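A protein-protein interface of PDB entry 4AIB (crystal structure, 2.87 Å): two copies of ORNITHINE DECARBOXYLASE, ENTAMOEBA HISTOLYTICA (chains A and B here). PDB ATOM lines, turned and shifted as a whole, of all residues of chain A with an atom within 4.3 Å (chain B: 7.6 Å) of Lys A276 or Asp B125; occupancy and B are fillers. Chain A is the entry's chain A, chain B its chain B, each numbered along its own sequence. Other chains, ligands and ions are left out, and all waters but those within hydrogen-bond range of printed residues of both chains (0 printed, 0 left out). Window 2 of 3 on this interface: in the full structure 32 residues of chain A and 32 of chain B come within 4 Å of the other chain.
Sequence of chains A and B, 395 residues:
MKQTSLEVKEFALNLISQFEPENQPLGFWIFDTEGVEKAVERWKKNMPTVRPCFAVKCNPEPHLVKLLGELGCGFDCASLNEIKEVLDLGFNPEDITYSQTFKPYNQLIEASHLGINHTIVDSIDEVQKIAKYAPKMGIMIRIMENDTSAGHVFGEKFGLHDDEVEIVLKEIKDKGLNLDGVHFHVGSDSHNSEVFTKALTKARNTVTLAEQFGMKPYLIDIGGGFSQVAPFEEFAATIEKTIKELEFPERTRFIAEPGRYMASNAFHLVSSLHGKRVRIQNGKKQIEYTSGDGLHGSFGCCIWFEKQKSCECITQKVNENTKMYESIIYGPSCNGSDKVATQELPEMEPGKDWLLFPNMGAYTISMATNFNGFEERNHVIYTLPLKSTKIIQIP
Printed residues of chain B within 4 Å of Lys A276: Phe B102, Ser B123 and Asp B125. Of chain A, only Lys A276 comes within 4 Å of Asp B125. Of the printed residues of chain A, Ser B123 touches Lys A276 and Arg A277. Of the printed residues of chain B, Pro A350 touches Tyr B105. Of the printed residues of chain A, Asp B122 touches Arg A277. Ile B130 touches none of the printed residues of chain A. The nearest residue of chain B that does not touch Lys A276 is Glu B126 (5.0 Å). The nearest residue of chain A that does not touch Asp B125 is Pro A350 (4.1 Å).
Among the printed residues, pairs that only touch across the chains: Gly A275 with Phe B102 (3.5 Å), Gly A275 with Lys B129 (3.95 Å), Lys A276 with Phe B102 (3.7 Å) and Arg A277 with Ser B123 (3.98 Å).
No position is printed for both chains. Of the 8 pairs that touch across the chains among the printed residues, none has its exchanged pair printed and touching as well.
The backbone carbonyl oxygen (O) of Met A348 sits close to the side-chain amino group (NZ) of Lys A276, 3.3 Å away. NH2 of Arg A277 is in salt-bridge range of OE1 of Glu A288, 2.6 Å away. The backbone carbonyl oxygen (O) of Lys B103 sits at hydrogen-bond distance from the side-chain amino group (NZ) of Lys B129. OG of Ser B123 is in hydrogen-bond range of N of Glu B126, at 3.4 Å. OE1 of Glu B126 lies within salt-bridge range of NZ of Lys B129 (2.8 Å).
The side-chain hydroxyl (OG) of Ser B123 is in hydrogen-bond range of the backbone carbonyl oxygen (O) of Lys A276, at 3.4 Å. The backbone NH of Lys A276 sits at hydrogen-bond distance from the side-chain carboxylate of Asp B125 (3.5 Å). The side-chain carboxylate (OD2) of Asp B122 lies within salt-bridge range of the guanidinium group (NH1) of Arg A277, 2.7 Å away. The backbone carbonyl oxygen (O) of Pro A350 is in hydrogen-bond range of the side-chain hydroxyl (OH) of Tyr B105, 2.9 Å away.
Hydrophobic or aromatic side chains of chain B within 4 Å of the printed part of chain A: Phe B102 and Tyr B105. Of the 9 printed residues of chain A, 4 touch a printed residue of chain B. Along chain A the printed residues that touch a printed residue of chain B span positions 275 to 350. Among the printed residues, 8 pairs touch across the chains.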
ATOM      1  N   GLY A 275     -10.213 -21.030  11.925  1.00  0.00           N
ATOM      2  CA  GLY A 275      -9.040 -20.707  11.116  1.00  0.00           C
ATOM      3  C   GLY A 275      -7.943 -19.975  11.869  1.00  0.00           C
ATOM      4  O   GLY A 275      -8.218 -19.083  12.676  1.00  0.00           O
ATOM      5  N   LYS A 276      -6.696 -20.351  11.593  1.00  0.00           N
ATOM      6  CA  LYS A 276      -5.536 -19.741  12.241  1.00  0.00           C
ATOM      7  C   LYS A 276      -4.318 -19.693  11.321  1.00  0.00           C
ATOM      8  O   LYS A 276      -4.063 -20.630  10.560  1.00  0.00           O
ATOM      9  CB  LYS A 276      -5.189 -20.488  13.535  1.00  0.00           C
ATOM     10  CG  LYS A 276      -4.266 -19.722  14.473  1.00  0.00           C
ATOM     11  CD  LYS A 276      -4.092 -20.425  15.811  1.00  0.00           C
ATOM     12  CE  LYS A 276      -3.006 -21.489  15.771  1.00  0.00           C
ATOM     13  NZ  LYS A 276      -2.771 -22.083  17.117  1.00  0.00           N
ATOM     14  N   ARG A 277      -3.572 -18.592  11.399  1.00  0.00           N
ATOM     15  CA  ARG A 277      -2.323 -18.435  10.660  1.00  0.00           C
ATOM     16  C   ARG A 277      -1.291 -17.665  11.484  1.00  0.00           C
ATOM     17  O   ARG A 277      -1.490 -16.492  11.810  1.00  0.00           O
ATOM     18  CB  ARG A 277      -2.567 -17.748   9.309  1.00  0.00           C
ATOM     19  CG  ARG A 277      -1.313 -17.558   8.467  1.00  0.00           C
ATOM     20  CD  ARG A 277      -1.638 -17.302   7.004  1.00  0.00           C
ATOM     21  NE  ARG A 277      -2.284 -16.007   6.784  1.00  0.00           N
ATOM     22  CZ  ARG A 277      -2.574 -15.505   5.586  1.00  0.00           C
ATOM     23  NH1 ARG A 277      -2.276 -16.181   4.482  1.00  0.00           N
ATOM     24  NH2 ARG A 277      -3.162 -14.321   5.486  1.00  0.00           N
ATOM     25  N   ILE A 287      -0.751 -13.277  15.004  1.00  0.00           N
ATOM     26  CA  ILE A 287      -1.583 -14.445  14.715  1.00  0.00           C
ATOM     27  C   ILE A 287      -2.932 -14.043  14.121  1.00  0.00           C
ATOM     28  O   ILE A 287      -3.716 -13.336  14.755  1.00  0.00           O
ATOM     29  CB  ILE A 287      -1.787 -15.342  15.958  1.00  0.00           C
ATOM     30  CG1 ILE A 287      -0.469 -15.521  16.724  1.00  0.00           C
ATOM     31  CG2 ILE A 287      -2.348 -16.696  15.540  1.00  0.00           C
ATOM     32  CD1 ILE A 287      -0.617 -16.123  18.106  1.00  0.00           C
ATOM     33  N   GLU A 288      -3.185 -14.503  12.898  1.00  0.00           N
ATOM     34  CA  GLU A 288      -4.440 -14.231  12.200  1.00  0.00           C
ATOM     35  C   GLU A 288      -5.500 -15.273  12.541  1.00  0.00           C
ATOM     36  O   GLU A 288      -5.218 -16.471  12.580  1.00  0.00           O
ATOM     37  CB  GLU A 288      -4.216 -14.186  10.686  1.00  0.00           C
ATOM     38  CG  GLU A 288      -3.536 -12.917  10.190  1.00  0.00           C
ATOM     39  CD  GLU A 288      -3.021 -13.039   8.767  1.00  0.00           C
ATOM     40  OE1 GLU A 288      -3.781 -13.506   7.892  1.00  0.00           O
ATOM     41  OE2 GLU A 288      -1.857 -12.656   8.518  1.00  0.00           O
ATOM     42  N   TYR A 289      -6.719 -14.805  12.790  1.00  0.00           N
ATOM     43  CA  TYR A 289      -7.832 -15.688  13.124  1.00  0.00           C
ATOM     44  C   TYR A 289      -9.016 -15.476  12.191  1.00  0.00           C
ATOM     45  O   TYR A 289      -9.215 -14.384  11.655  1.00  0.00           O
ATOM     46  CB  TYR A 289      -8.262 -15.486  14.578  1.00  0.00           C
ATOM     47  CG  TYR A 289      -7.218 -15.900  15.590  1.00  0.00           C
ATOM     48  CD1 TYR A 289      -7.100 -17.230  15.994  1.00  0.00           C
ATOM     49  CD2 TYR A 289      -6.350 -14.963  16.148  1.00  0.00           C
ATOM     50  CE1 TYR A 289      -6.145 -17.615  16.922  1.00  0.00           C
ATOM     51  CE2 TYR A 289      -5.391 -15.338  17.077  1.00  0.00           C
ATOM     52  CZ  TYR A 289      -5.295 -16.663  17.461  1.00  0.00           C
ATOM     53  OH  TYR A 289      -4.344 -17.039  18.382  1.00  0.00           O
ATOM     54  N   GLU A 347      -2.701 -16.630  22.505  1.00  0.00           N
ATOM     55  CA  GLU A 347      -2.744 -17.635  21.445  1.00  0.00           C
ATOM     56  C   GLU A 347      -3.951 -18.550  21.634  1.00  0.00           C
ATOM     57  O   GLU A 347      -4.140 -19.133  22.704  1.00  0.00           O
ATOM     58  CB  GLU A 347      -1.447 -18.452  21.403  1.00  0.00           C
ATOM     59  CG  GLU A 347      -1.302 -19.323  20.161  1.00  0.00           C
ATOM     60  CD  GLU A 347      -0.106 -20.256  20.219  1.00  0.00           C
ATOM     61  OE1 GLU A 347       0.203 -20.778  21.312  1.00  0.00           O
ATOM     62  OE2 GLU A 347       0.521 -20.478  19.162  1.00  0.00           O
ATOM     63  N   MET A 348      -4.765 -18.658  20.588  1.00  0.00           N
ATOM     64  CA  MET A 348      -6.012 -19.411  20.650  1.00  0.00           C
ATOM     65  C   MET A 348      -5.987 -20.648  19.758  1.00  0.00           C
ATOM     66  O   MET A 348      -5.240 -20.707  18.781  1.00  0.00           O
ATOM     67  CB  MET A 348      -7.195 -18.513  20.282  1.00  0.00           C
ATOM     68  CG  MET A 348      -7.495 -17.433  21.309  1.00  0.00           C
ATOM     69  SD  MET A 348      -8.852 -16.344  20.838  1.00  0.00           S
ATOM     70  CE  MET A 348      -8.077 -15.325  19.584  1.00  0.00           C
ATOM     71  N   PRO A 350      -8.399 -22.982  17.379  1.00  0.00           N
ATOM     72  CA  PRO A 350      -9.679 -23.053  16.667  1.00  0.00           C
ATOM     73  C   PRO A 350     -10.436 -24.341  16.979  1.00  0.00           C
ATOM     74  O   PRO A 350      -9.866 -25.433  16.899  1.00  0.00           O
ATOM     75  CB  PRO A 350      -9.267 -23.015  15.188  1.00  0.00           C
ATOM     76  CG  PRO A 350      -7.902 -22.421  15.181  1.00  0.00           C
ATOM     77  CD  PRO A 350      -7.262 -22.906  16.446  1.00  0.00           C
ATOM     78  N   THR B 101     -10.183 -20.599   2.129  1.00  0.00           N
ATOM     79  CA  THR B 101      -8.911 -20.697   2.840  1.00  0.00           C
ATOM     80  C   THR B 101      -9.096 -21.211   4.264  1.00  0.00           C
ATOM     81  O   THR B 101      -8.290 -22.002   4.747  1.00  0.00           O
ATOM     82  CB  THR B 101      -8.167 -19.346   2.878  1.00  0.00           C
ATOM     83  OG1 THR B 101      -9.069 -18.310   3.290  1.00  0.00           O
ATOM     84  CG2 THR B 101      -7.595 -19.003   1.509  1.00  0.00           C
ATOM     85  N   PHE B 102     -10.162 -20.762   4.923  1.00  0.00           N
ATOM     86  CA  PHE B 102     -10.458 -21.176   6.292  1.00  0.00           C
ATOM     87  C   PHE B 102     -11.892 -21.685   6.419  1.00  0.00           C
ATOM     88  O   PHE B 102     -12.842 -20.902   6.506  1.00  0.00           O
ATOM     89  CB  PHE B 102     -10.186 -20.031   7.273  1.00  0.00           C
ATOM     90  CG  PHE B 102      -8.763 -19.540   7.252  1.00  0.00           C
ATOM     91  CD1 PHE B 102      -7.764 -20.233   7.928  1.00  0.00           C
ATOM     92  CD2 PHE B 102      -8.421 -18.386   6.554  1.00  0.00           C
ATOM     93  CE1 PHE B 102      -6.454 -19.783   7.914  1.00  0.00           C
ATOM     94  CE2 PHE B 102      -7.111 -17.931   6.534  1.00  0.00           C
ATOM     95  CZ  PHE B 102      -6.125 -18.632   7.214  1.00  0.00           C
ATOM     96  N   LYS B 103     -12.027 -23.009   6.425  1.00  0.00           N
ATOM     97  CA  LYS B 103     -13.328 -23.673   6.421  1.00  0.00           C
ATOM     98  C   LYS B 103     -13.780 -24.058   7.828  1.00  0.00           C
ATOM     99  O   LYS B 103     -12.968 -24.519   8.634  1.00  0.00           O
ATOM    100  CB  LYS B 103     -13.278 -24.926   5.539  1.00  0.00           C
ATOM    101  CG  LYS B 103     -12.942 -24.657   4.079  1.00  0.00           C
ATOM    102  CD  LYS B 103     -12.554 -25.924   3.331  1.00  0.00           C
ATOM    103  CE  LYS B 103     -11.122 -26.351   3.624  1.00  0.00           C
ATOM    104  NZ  LYS B 103     -10.114 -25.375   3.119  1.00  0.00           N
ATOM    105  N   TYR B 105     -15.390 -26.473  10.569  1.00  0.00           N
ATOM    106  CA  TYR B 105     -15.227 -27.920  10.725  1.00  0.00           C
ATOM    107  C   TYR B 105     -16.450 -28.711  10.258  1.00  0.00           C
ATOM    108  O   TYR B 105     -16.314 -29.677   9.506  1.00  0.00           O
ATOM    109  CB  TYR B 105     -14.885 -28.274  12.176  1.00  0.00           C
ATOM    110  CG  TYR B 105     -13.594 -27.664  12.680  1.00  0.00           C
ATOM    111  CD1 TYR B 105     -12.367 -28.279  12.433  1.00  0.00           C
ATOM    112  CD2 TYR B 105     -13.599 -26.475  13.410  1.00  0.00           C
ATOM    113  CE1 TYR B 105     -11.182 -27.728  12.896  1.00  0.00           C
ATOM    114  CE2 TYR B 105     -12.418 -25.914  13.876  1.00  0.00           C
ATOM    115  CZ  TYR B 105     -11.214 -26.544  13.613  1.00  0.00           C
ATOM    116  OH  TYR B 105     -10.037 -25.998  14.071  1.00  0.00           O
ATOM    117  N   VAL B 121      -5.847 -24.024   0.206  1.00  0.00           N
ATOM    118  CA  VAL B 121      -5.167 -23.788   1.484  1.00  0.00           C
ATOM    119  C   VAL B 121      -4.108 -22.689   1.371  1.00  0.00           C
ATOM    120  O   VAL B 121      -3.471 -22.534   0.326  1.00  0.00           O
ATOM    121  CB  VAL B 121      -4.551 -25.099   2.037  1.00  0.00           C
ATOM    122  CG1 VAL B 121      -3.231 -24.858   2.758  1.00  0.00           C
ATOM    123  CG2 VAL B 121      -5.538 -25.791   2.958  1.00  0.00           C
ATOM    124  N   ASP B 122      -3.934 -21.929   2.453  1.00  0.00           N
ATOM    125  CA  ASP B 122      -2.910 -20.886   2.523  1.00  0.00           C
ATOM    126  C   ASP B 122      -2.177 -20.858   3.869  1.00  0.00           C
ATOM    127  O   ASP B 122      -1.224 -20.095   4.042  1.00  0.00           O
ATOM    128  CB  ASP B 122      -3.523 -19.511   2.226  1.00  0.00           C
ATOM    129  CG  ASP B 122      -4.347 -18.974   3.384  1.00  0.00           C
ATOM    130  OD1 ASP B 122      -5.042 -19.768   4.055  1.00  0.00           O
ATOM    131  OD2 ASP B 122      -4.300 -17.748   3.622  1.00  0.00           O
ATOM    132  N   SER B 123      -2.630 -21.678   4.817  1.00  0.00           N
ATOM    133  CA  SER B 123      -2.033 -21.732   6.154  1.00  0.00           C
ATOM    134  C   SER B 123      -1.702 -23.164   6.572  1.00  0.00           C
ATOM    135  O   SER B 123      -2.314 -24.117   6.083  1.00  0.00           O
ATOM    136  CB  SER B 123      -2.963 -21.086   7.186  1.00  0.00           C
ATOM    137  OG  SER B 123      -4.087 -21.909   7.452  1.00  0.00           O
ATOM    138  N   ILE B 124      -0.743 -23.307   7.484  1.00  0.00           N
ATOM    139  CA  ILE B 124      -0.322 -24.630   7.961  1.00  0.00           C
ATOM    140  C   ILE B 124      -1.397 -25.314   8.814  1.00  0.00           C
ATOM    141  O   ILE B 124      -1.461 -26.543   8.867  1.00  0.00           O
ATOM    142  CB  ILE B 124       1.036 -24.595   8.714  1.00  0.00           C
ATOM    143  CG1 ILE B 124       0.893 -23.946  10.101  1.00  0.00           C
ATOM    144  CG2 ILE B 124       2.098 -23.882   7.882  1.00  0.00           C
ATOM    145  CD1 ILE B 124       1.859 -24.483  11.138  1.00  0.00           C
ATOM    146  N   ASP B 125      -2.238 -24.509   9.467  1.00  0.00           N
ATOM    147  CA  ASP B 125      -3.312 -25.006  10.330  1.00  0.00           C
ATOM    148  C   ASP B 125      -4.420 -25.695   9.536  1.00  0.00           C
ATOM    149  O   ASP B 125      -4.924 -26.744   9.945  1.00  0.00           O
ATOM    150  CB  ASP B 125      -3.895 -23.859  11.167  1.00  0.00           C
ATOM    151  CG  ASP B 125      -5.085 -24.289  12.012  1.00  0.00           C
ATOM    152  OD1 ASP B 125      -4.908 -25.129  12.920  1.00  0.00           O
ATOM    153  OD2 ASP B 125      -6.202 -23.785  11.763  1.00  0.00           O
ATOM    154  N   GLU B 126      -4.788 -25.103   8.402  1.00  0.00           N
ATOM    155  CA  GLU B 126      -5.847 -25.638   7.545  1.00  0.00           C
ATOM    156  C   GLU B 126      -5.461 -26.983   6.922  1.00  0.00           C
ATOM    157  O   GLU B 126      -6.331 -27.794   6.596  1.00  0.00           O
ATOM    158  CB  GLU B 126      -6.220 -24.626   6.458  1.00  0.00           C
ATOM    159  CG  GLU B 126      -7.566 -24.883   5.789  1.00  0.00           C
ATOM    160  CD  GLU B 126      -8.758 -24.474   6.640  1.00  0.00           C
ATOM    161  OE1 GLU B 126      -8.582 -23.728   7.628  1.00  0.00           O
ATOM    162  OE2 GLU B 126      -9.885 -24.892   6.308  1.00  0.00           O
ATOM    163  N   VAL B 127      -4.158 -27.208   6.764  1.00  0.00           N
ATOM    164  CA  VAL B 127      -3.633 -28.490   6.290  1.00  0.00           C
ATOM    165  C   VAL B 127      -3.955 -29.586   7.304  1.00  0.00           C
ATOM    166  O   VAL B 127      -4.456 -30.652   6.943  1.00  0.00           O
ATOM    167  CB  VAL B 127      -2.104 -28.437   6.066  1.00  0.00           C
ATOM    168  CG1 VAL B 127      -1.603 -29.737   5.453  1.00  0.00           C
ATOM    169  CG2 VAL B 127      -1.725 -27.256   5.187  1.00  0.00           C
ATOM    170  N   GLN B 128      -3.672 -29.299   8.575  1.00  0.00           N
ATOM    171  CA  GLN B 128      -3.908 -30.232   9.675  1.00  0.00           C
ATOM    172  C   GLN B 128      -5.397 -30.491   9.891  1.00  0.00           C
ATOM    173  O   GLN B 128      -5.789 -31.590  10.282  1.00  0.00           O
ATOM    174  CB  GLN B 128      -3.276 -29.700  10.963  1.00  0.00           C
ATOM    175  CG  GLN B 128      -1.771 -29.487  10.875  1.00  0.00           C
ATOM    176  CD  GLN B 128      -1.225 -28.638  12.009  1.00  0.00           C
ATOM    177  OE1 GLN B 128      -1.864 -27.684  12.456  1.00  0.00           O
ATOM    178  NE2 GLN B 128      -0.029 -28.978  12.474  1.00  0.00           N
ATOM    179  N   LYS B 129      -6.211 -29.467   9.634  1.00  0.00           N
ATOM    180  CA  LYS B 129      -7.669 -29.555   9.720  1.00  0.00           C
ATOM    181  C   LYS B 129      -8.224 -30.523   8.673  1.00  0.00           C
ATOM    182  O   LYS B 129      -9.042 -31.390   8.988  1.00  0.00           O
ATOM    183  CB  LYS B 129      -8.285 -28.166   9.535  1.00  0.00           C
ATOM    184  CG  LYS B 129      -9.801 -28.106   9.671  1.00  0.00           C
ATOM    185  CD  LYS B 129     -10.352 -26.753   9.241  1.00  0.00           C
ATOM    186  CE  LYS B 129      -9.930 -25.634  10.184  1.00  0.00           C
ATOM    187  NZ  LYS B 129     -10.387 -24.300   9.708  1.00  0.00           N
ATOM    188  N   ILE B 130      -7.768 -30.363   7.432  1.00  0.00           N
ATOM    189  CA  ILE B 130      -8.183 -31.220   6.322  1.00  0.00           C
ATOM    190  C   ILE B 130      -7.694 -32.656   6.528  1.00  0.00           C
ATOM    191  O   ILE B 130      -8.415 -33.607   6.236  1.00  0.00           O
ATOM    192  CB  ILE B 130      -7.724 -30.638   4.963  1.00  0.00           C
ATOM    193  CG1 ILE B 130      -8.553 -29.393   4.629  1.00  0.00           C
ATOM    194  CG2 ILE B 130      -7.851 -31.664   3.842  1.00  0.00           C
ATOM    195  CD1 ILE B 130      -7.918 -28.467   3.614  1.00  0.00           C
ATOM    196  N   ALA B 131      -6.481 -32.800   7.058  1.00  0.00           N
ATOM    197  CA  ALA B 131      -5.918 -34.115   7.379  1.00  0.00           C
ATOM    198  C   ALA B 131      -6.686 -34.828   8.497  1.00  0.00           C
ATOM    199  O   ALA B 131      -6.726 -36.061   8.543  1.00  0.00           O
ATOM    200  CB  ALA B 131      -4.447 -33.984   7.745  1.00  0.00           C
ATOM    201  N   VAL B 168       4.301 -25.013   4.013  1.00  0.00           N
ATOM    202  CA  VAL B 168       2.984 -25.623   3.802  1.00  0.00           C
ATOM    203  C   VAL B 168       3.089 -26.931   3.011  1.00  0.00           C
ATOM    204  O   VAL B 168       2.502 -27.940   3.406  1.00  0.00           O
ATOM    205  CB  VAL B 168       1.999 -24.642   3.114  1.00  0.00           C
ATOM    206  CG1 VAL B 168       0.648 -25.301   2.869  1.00  0.00           C
ATOM    207  CG2 VAL B 168       1.823 -23.384   3.954  1.00  0.00           C
ATOM    208  N   GLU B 171       4.122 -29.793   5.058  1.00  0.00           N
ATOM    209  CA  GLU B 171       3.001 -30.235   5.887  1.00  0.00           C
ATOM    210  C   GLU B 171       1.988 -31.066   5.092  1.00  0.00           C
ATOM    211  O   GLU B 171       1.428 -32.025   5.623  1.00  0.00           O
ATOM    212  CB  GLU B 171       2.317 -29.037   6.560  1.00  0.00           C
ATOM    213  CG  GLU B 171       1.332 -29.391   7.671  1.00  0.00           C
ATOM    214  CD  GLU B 171       1.991 -29.625   9.021  1.00  0.00           C
ATOM    215  OE1 GLU B 171       2.964 -30.405   9.100  1.00  0.00           O
ATOM    216  OE2 GLU B 171       1.517 -29.034  10.015  1.00  0.00           O
